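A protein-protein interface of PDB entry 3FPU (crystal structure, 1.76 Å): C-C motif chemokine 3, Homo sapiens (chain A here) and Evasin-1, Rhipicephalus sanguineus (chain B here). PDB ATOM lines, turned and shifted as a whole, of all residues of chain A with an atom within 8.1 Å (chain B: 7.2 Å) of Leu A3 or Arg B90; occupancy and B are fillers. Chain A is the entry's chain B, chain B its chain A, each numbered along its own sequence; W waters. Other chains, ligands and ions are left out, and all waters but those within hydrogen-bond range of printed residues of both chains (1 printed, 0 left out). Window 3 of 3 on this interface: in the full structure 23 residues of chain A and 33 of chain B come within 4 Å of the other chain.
Water W1 lies within hydrogen-bond range of the backbone NH (N) of Arg B87 and the side-chain hydroxyl (OG1) of Thr A9.
The side-chain carboxylate (OD2) of Asp B91 lies within hydrogen-bond range of the backbone NH (N) of Asn B88.
The backbone carbonyl oxygen (O) of Ala A4 is in hydrogen-bond range of the side-chain hydroxyl (OG1) of Thr A7, 2.6 Å away.
The side-chain hydroxyl of Thr A7 is in hydrogen-bond range of the side-chain amide nitrogen of Gln A49 (3.0 Å).
The backbone NH of Thr A9 is in hydrogen-bond range of the backbone carbonyl oxygen of Arg B87 (3.0 Å).
The side-chain amide oxygen (OD1) of Asn B88 lies close to the backbone carbonyl oxygen (O) of Asp A6.
O of Thr A7 sits close to OD1 of Asn B88 (3.3 Å).
The backbone carbonyl oxygen (O) of Ala A5 sits at hydrogen-bond distance from the backbone NH (N) of Trp B89, at 3.2 Å.
The backbone carbonyl oxygen (O) of Thr A7 lies within hydrogen-bond range of the backbone NH (N) of Trp B89, 3.1 Å away.
The indole nitrogen of Trp B89 sits at hydrogen-bond distance from the side-chain amide oxygen of Gln A49 (3.2 Å).
N of Arg B90 sits at hydrogen-bond distance from O of Ala A5, 2.8 Å away.
NE of Arg B90 is in salt-bridge range of OD1 of Asp A6.
The backbone nitrogen (N) of Pro A8 lies close to the side-chain amide oxygen (OD1) of Asn B88, 3.4 Å away.
Leu A3 touches Arg B90.
Trp B89 touches Ala A4.
Asn B88 touches Ala A5 (CB to O, 3.6 Å).
Lys B93 touches Ala A5 (NZ to CB, 3.5 Å).
Pro A8 touches Arg B87 (CA to O, 3.4 Å).
Trp B89 touches Pro A8.
Thr A9 touches Asn B88.
CA of Thr A9 touches CZ2 of Trp B89 (3.8 Å).
CG of Lys B92 touches CG2 of Thr A9 (3.9 Å).
Trp B89 touches Phe A29.
Leu A3 touches just one residue of chain B: Arg B90 (3.5 Å).
Of chain A, only Leu A3 (3.5 Å), Ala A5 (2.8 Å) and Asp A6 (2.6 Å) come within 4 Å of Arg B90.
Of the printed residues of chain B, Phe A29 touches Trp B89 (3.6 Å).
Of the printed residues of chain A, Lys B93 touches Ala A5 (3.5 Å).
Of the printed residues of chain B, Ala A5 touches Asn B88 (3.6 Å), Trp B89 (3.2 Å), Arg B90 (2.8 Å) and Lys B93 (3.5 Å).
Asp B91 touches none of the printed residues of chain A.
The nearest residue of chain B that does not touch Leu A3 is Trp B89 (6.9 Å).
Printed residues of chain A that touch a printed residue of chain B: Leu A3, Ala A4, Ala A5, Asp A6, Thr A7, Pro A8, Thr A9, Phe A29 and Gln A49.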
ATOM      1  N   SER A   2      19.406   4.634   8.364  1.00  0.00           N
ATOM      2  CA  SER A   2      19.235   5.889   9.177  1.00  0.00           C
ATOM      3  C   SER A   2      17.913   5.989   9.969  1.00  0.00           C
ATOM      4  O   SER A   2      17.846   6.729  10.951  1.00  0.00           O
ATOM      5  CB  SER A   2      19.509   7.136   8.330  1.00  0.00           C
ATOM      6  OG  SER A   2      20.905   7.275   8.127  1.00  0.00           O
ATOM      7  N   LEU A   3      16.858   5.279   9.553  1.00  0.00           N
ATOM      8  CA  LEU A   3      16.761   4.709   8.231  1.00  0.00           C
ATOM      9  C   LEU A   3      15.988   5.743   7.418  1.00  0.00           C
ATOM     10  O   LEU A   3      15.002   6.356   7.904  1.00  0.00           O
ATOM     11  CB  LEU A   3      16.086   3.327   8.244  1.00  0.00           C
ATOM     12  CG  LEU A   3      16.757   2.173   9.024  1.00  0.00           C
ATOM     13  CD1 LEU A   3      15.802   1.056   9.406  1.00  0.00           C
ATOM     14  CD2 LEU A   3      17.959   1.580   8.264  1.00  0.00           C
ATOM     15  N   ALA A   4      16.421   5.941   6.180  1.00  0.00           N
ATOM     16  CA  ALA A   4      15.801   6.963   5.341  1.00  0.00           C
ATOM     17  C   ALA A   4      14.350   6.598   5.041  1.00  0.00           C
ATOM     18  O   ALA A   4      13.509   7.496   4.859  1.00  0.00           O
ATOM     19  CB  ALA A   4      16.553   7.129   4.064  1.00  0.00           C
ATOM     20  N   ALA A   5      14.064   5.304   4.958  1.00  0.00           N
ATOM     21  CA  ALA A   5      12.677   4.846   4.726  1.00  0.00           C
ATOM     22  C   ALA A   5      11.720   5.279   5.823  1.00  0.00           C
ATOM     23  O   ALA A   5      10.507   5.287   5.618  1.00  0.00           O
ATOM     24  CB  ALA A   5      12.608   3.334   4.533  1.00  0.00           C
ATOM     25  N   ASP A   6      12.251   5.667   6.975  1.00  0.00           N
ATOM     26  CA  ASP A   6      11.405   6.126   8.078  1.00  0.00           C
ATOM     27  C   ASP A   6      11.332   7.641   8.202  1.00  0.00           C
ATOM     28  O   ASP A   6      10.929   8.160   9.258  1.00  0.00           O
ATOM     29  CB  ASP A   6      11.837   5.462   9.390  1.00  0.00           C
ATOM     30  CG  ASP A   6      11.687   3.959   9.329  1.00  0.00           C
ATOM     31  OD1 ASP A   6      10.682   3.489   8.743  1.00  0.00           O
ATOM     32  OD2 ASP A   6      12.575   3.233   9.827  1.00  0.00           O
ATOM     33  N   THR A   7      11.735   8.354   7.138  1.00  0.00           N
ATOM     34  CA  THR A   7      11.575   9.794   7.129  1.00  0.00           C
ATOM     35  C   THR A   7      10.275  10.118   6.357  1.00  0.00           C
ATOM     36  O   THR A   7       9.784   9.245   5.640  1.00  0.00           O
ATOM     37  CB  THR A   7      12.777  10.536   6.488  1.00  0.00           C
ATOM     38  OG1 THR A   7      12.981  10.075   5.152  1.00  0.00           O
ATOM     39  CG2 THR A   7      14.047  10.303   7.321  1.00  0.00           C
ATOM     40  N   PRO A   8       9.730  11.319   6.550  1.00  0.00           N
ATOM     41  CA  PRO A   8       8.422  11.611   5.957  1.00  0.00           C
ATOM     42  C   PRO A   8       8.430  11.717   4.447  1.00  0.00           C
ATOM     43  O   PRO A   8       9.430  12.127   3.837  1.00  0.00           O
ATOM     44  CB  PRO A   8       8.054  12.979   6.564  1.00  0.00           C
ATOM     45  CG  PRO A   8       8.827  13.046   7.836  1.00  0.00           C
ATOM     46  CD  PRO A   8      10.153  12.416   7.434  1.00  0.00           C
ATOM     47  N   THR A   9       7.291  11.374   3.849  1.00  0.00           N
ATOM     48  CA  THR A   9       7.093  11.562   2.418  1.00  0.00           C
ATOM     49  C   THR A   9       7.161  13.060   2.084  1.00  0.00           C
ATOM     50  O   THR A   9       6.890  13.900   2.931  1.00  0.00           O
ATOM     51  CB  THR A   9       5.717  11.005   1.932  1.00  0.00           C
ATOM     52  OG1 THR A   9       4.685  11.626   2.710  1.00  0.00           O
ATOM     53  CG2 THR A   9       5.656   9.483   2.190  1.00  0.00           C
ATOM     54  N   PHE A  29      13.296   7.336  -3.836  1.00  0.00           N
ATOM     55  CA  PHE A  29      11.889   7.206  -3.467  1.00  0.00           C
ATOM     56  C   PHE A  29      11.101   7.899  -4.562  1.00  0.00           C
ATOM     57  O   PHE A  29      11.588   8.845  -5.173  1.00  0.00           O
ATOM     58  CB  PHE A  29      11.637   7.888  -2.124  1.00  0.00           C
ATOM     59  CG  PHE A  29      12.487   7.355  -1.022  1.00  0.00           C
ATOM     60  CD1 PHE A  29      12.320   6.050  -0.552  1.00  0.00           C
ATOM     61  CD2 PHE A  29      13.447   8.168  -0.428  1.00  0.00           C
ATOM     62  CE1 PHE A  29      13.132   5.568   0.481  1.00  0.00           C
ATOM     63  CE2 PHE A  29      14.265   7.692   0.597  1.00  0.00           C
ATOM     64  CZ  PHE A  29      14.098   6.413   1.061  1.00  0.00           C
ATOM     65  N   LEU A  43      18.454   9.732  -2.694  1.00  0.00           N
ATOM     66  CA  LEU A  43      19.067   9.799  -1.369  1.00  0.00           C
ATOM     67  C   LEU A  43      20.562   9.640  -1.664  1.00  0.00           C
ATOM     68  O   LEU A  43      20.961   8.637  -2.274  1.00  0.00           O
ATOM     69  CB  LEU A  43      18.547   8.636  -0.538  1.00  0.00           C
ATOM     70  CG  LEU A  43      19.210   8.463   0.853  1.00  0.00           C
ATOM     71  CD1 LEU A  43      18.670   9.552   1.716  1.00  0.00           C
ATOM     72  CD2 LEU A  43      18.942   7.076   1.420  1.00  0.00           C
ATOM     73  N   SER A  47      23.069  11.173   3.004  1.00  0.00           N
ATOM     74  CA  SER A  47      21.692  11.237   3.573  1.00  0.00           C
ATOM     75  C   SER A  47      20.878  12.456   3.165  1.00  0.00           C
ATOM     76  O   SER A  47      19.827  12.751   3.783  1.00  0.00           O
ATOM     77  CB  SER A  47      21.708  11.178   5.109  1.00  0.00           C
ATOM     78  OG  SER A  47      22.350  10.018   5.539  1.00  0.00           O
ATOM     79  N   GLN A  49      18.285  14.222   0.750  1.00  0.00           N
ATOM     80  CA  GLN A  49      17.217  13.872  -0.195  1.00  0.00           C
ATOM     81  C   GLN A  49      17.057  15.033  -1.178  1.00  0.00           C
ATOM     82  O   GLN A  49      16.916  16.211  -0.762  1.00  0.00           O
ATOM     83  CB  GLN A  49      15.911  13.533   0.575  1.00  0.00           C
ATOM     84  CG  GLN A  49      16.090  12.259   1.342  1.00  0.00           C
ATOM     85  CD  GLN A  49      14.867  11.783   2.109  1.00  0.00           C
ATOM     86  OE1 GLN A  49      13.734  12.002   1.686  1.00  0.00           O
ATOM     87  NE2 GLN A  49      15.104  11.094   3.232  1.00  0.00           N
ATOM     88  N   ARG B  87       3.038  10.158   6.911  1.00  0.00           N
ATOM     89  CA  ARG B  87       3.399   8.852   6.343  1.00  0.00           C
ATOM     90  C   ARG B  87       4.888   8.905   6.137  1.00  0.00           C
ATOM     91  O   ARG B  87       5.409   9.962   5.751  1.00  0.00           O
ATOM     92  CB  ARG B  87       2.837   8.723   4.952  1.00  0.00           C
ATOM     93  CG  ARG B  87       1.455   9.233   4.841  1.00  0.00           C
ATOM     94  CD  ARG B  87       0.586   8.182   5.417  1.00  0.00           C
ATOM     95  NE  ARG B  87      -0.841   8.460   5.114  1.00  0.00           N
ATOM     96  CZ  ARG B  87      -1.832   8.030   5.883  1.00  0.00           C
ATOM     97  NH1 ARG B  87      -1.541   7.319   6.934  1.00  0.00           N
ATOM     98  NH2 ARG B  87      -3.111   8.280   5.598  1.00  0.00           N
ATOM     99  N   ASN B  88       5.568   7.768   6.279  1.00  0.00           N
ATOM    100  CA  ASN B  88       6.978   7.781   5.889  1.00  0.00           C
ATOM    101  C   ASN B  88       7.138   6.961   4.627  1.00  0.00           C
ATOM    102  O   ASN B  88       6.211   6.227   4.230  1.00  0.00           O
ATOM    103  CB  ASN B  88       7.800   7.146   7.005  1.00  0.00           C
ATOM    104  CG  ASN B  88       7.693   7.905   8.288  1.00  0.00           C
ATOM    105  OD1 ASN B  88       7.835   9.110   8.306  1.00  0.00           O
ATOM    106  ND2 ASN B  88       7.439   7.189   9.404  1.00  0.00           N
ATOM    107  N   TRP B  89       8.328   7.013   4.015  1.00  0.00           N
ATOM    108  CA  TRP B  89       8.523   6.269   2.772  1.00  0.00           C
ATOM    109  C   TRP B  89       8.186   4.778   2.893  1.00  0.00           C
ATOM    110  O   TRP B  89       7.638   4.197   1.965  1.00  0.00           O
ATOM    111  CB  TRP B  89       9.974   6.410   2.286  1.00  0.00           C
ATOM    112  CG  TRP B  89      10.320   7.843   1.949  1.00  0.00           C
ATOM    113  CD1 TRP B  89      11.277   8.602   2.540  1.00  0.00           C
ATOM    114  CD2 TRP B  89       9.743   8.656   0.910  1.00  0.00           C
ATOM    115  NE1 TRP B  89      11.335   9.851   1.951  1.00  0.00           N
ATOM    116  CE2 TRP B  89      10.404   9.911   0.949  1.00  0.00           C
ATOM    117  CE3 TRP B  89       8.741   8.453  -0.058  1.00  0.00           C
ATOM    118  CZ2 TRP B  89      10.082  10.968   0.077  1.00  0.00           C
ATOM    119  CZ3 TRP B  89       8.416   9.525  -0.928  1.00  0.00           C
ATOM    120  CH2 TRP B  89       9.094  10.748  -0.851  1.00  0.00           C
ATOM    121  N   ARG B  90       8.489   4.210   4.042  1.00  0.00           N
ATOM    122  CA  ARG B  90       8.236   2.783   4.299  1.00  0.00           C
ATOM    123  C   ARG B  90       6.785   2.417   4.065  1.00  0.00           C
ATOM    124  O   ARG B  90       6.475   1.292   3.660  1.00  0.00           O
ATOM    125  CB  ARG B  90       8.708   2.416   5.718  1.00  0.00           C
ATOM    126  CG  ARG B  90       8.828   0.913   5.965  1.00  0.00           C
ATOM    127  CD  ARG B  90       9.344   0.623   7.388  1.00  0.00           C
ATOM    128  NE  ARG B  90      10.653   1.196   7.625  1.00  0.00           N
ATOM    129  CZ  ARG B  90      11.802   0.687   7.165  1.00  0.00           C
ATOM    130  NH1 ARG B  90      11.827  -0.425   6.426  1.00  0.00           N
ATOM    131  NH2 ARG B  90      12.927   1.300   7.434  1.00  0.00           N
ATOM    132  N   ASP B  91       5.884   3.380   4.293  1.00  0.00           N
ATOM    133  CA  ASP B  91       4.446   3.139   4.176  1.00  0.00           C
ATOM    134  C   ASP B  91       3.950   3.007   2.725  1.00  0.00           C
ATOM    135  O   ASP B  91       2.829   2.565   2.487  1.00  0.00           O
ATOM    136  CB  ASP B  91       3.676   4.245   4.915  1.00  0.00           C
ATOM    137  CG  ASP B  91       3.955   4.239   6.396  1.00  0.00           C
ATOM    138  OD1 ASP B  91       3.899   3.149   7.042  1.00  0.00           O
ATOM    139  OD2 ASP B  91       4.237   5.319   6.991  1.00  0.00           O
ATOM    140  N   LYS B  92       4.815   3.375   1.788  1.00  0.00           N
ATOM    141  CA  LYS B  92       4.461   3.500   0.382  1.00  0.00           C
ATOM    142  C   LYS B  92       5.102   2.389  -0.446  1.00  0.00           C
ATOM    143  O   LYS B  92       4.759   2.233  -1.618  1.00  0.00           O
ATOM    144  CB  LYS B  92       4.963   4.854  -0.151  1.00  0.00           C
ATOM    145  CG  LYS B  92       4.423   6.105   0.560  1.00  0.00           C
ATOM    146  CD  LYS B  92       2.912   6.015   0.755  1.00  0.00           C
ATOM    147  CE  LYS B  92       2.324   7.338   1.168  1.00  0.00           C
ATOM    148  NZ  LYS B  92       1.897   8.104  -0.072  1.00  0.00           N
ATOM    149  N   LYS B  93       6.018   1.627   0.159  1.00  0.00           N
ATOM    150  CA  LYS B  93       6.949   0.727  -0.581  1.00  0.00           C
ATOM    151  C   LYS B  93       6.512  -0.722  -0.761  1.00  0.00           C
ATOM    152  O   LYS B  93       5.615  -1.187  -0.073  1.00  0.00           O
ATOM    153  CB  LYS B  93       8.331   0.722   0.080  1.00  0.00           C
ATOM    154  CG  LYS B  93       8.422  -0.167   1.320  1.00  0.00           C
ATOM    155  CD  LYS B  93       9.866  -0.464   1.746  1.00  0.00           C
ATOM    156  CE  LYS B  93      10.533   0.723   2.433  1.00  0.00           C
ATOM    157  NZ  LYS B  93      11.479   0.233   3.480  1.00  0.00           N
ATOM    158  N   ASN B  94       7.186  -1.408  -1.697  1.00  0.00           N
ATOM    159  CA  ASN B  94       7.117  -2.868  -1.928  1.00  0.00           C
ATOM    160  C   ASN B  94       5.708  -3.437  -2.171  1.00  0.00           C
ATOM    161  O   ASN B  94       4.735  -2.668  -2.263  1.00  0.00           O
ATOM    162  CB  ASN B  94       7.868  -3.641  -0.825  1.00  0.00           C
ATOM    163  CG  ASN B  94       9.326  -3.183  -0.652  1.00  0.00           C
ATOM    164  OD1 ASN B  94       9.859  -2.397  -1.446  1.00  0.00           O
ATOM    165  ND2 ASN B  94       9.977  -3.686   0.395  1.00  0.00           N
HETATM  166  O   HOH W   1       3.753  12.356   5.362  1.00  0.00           O
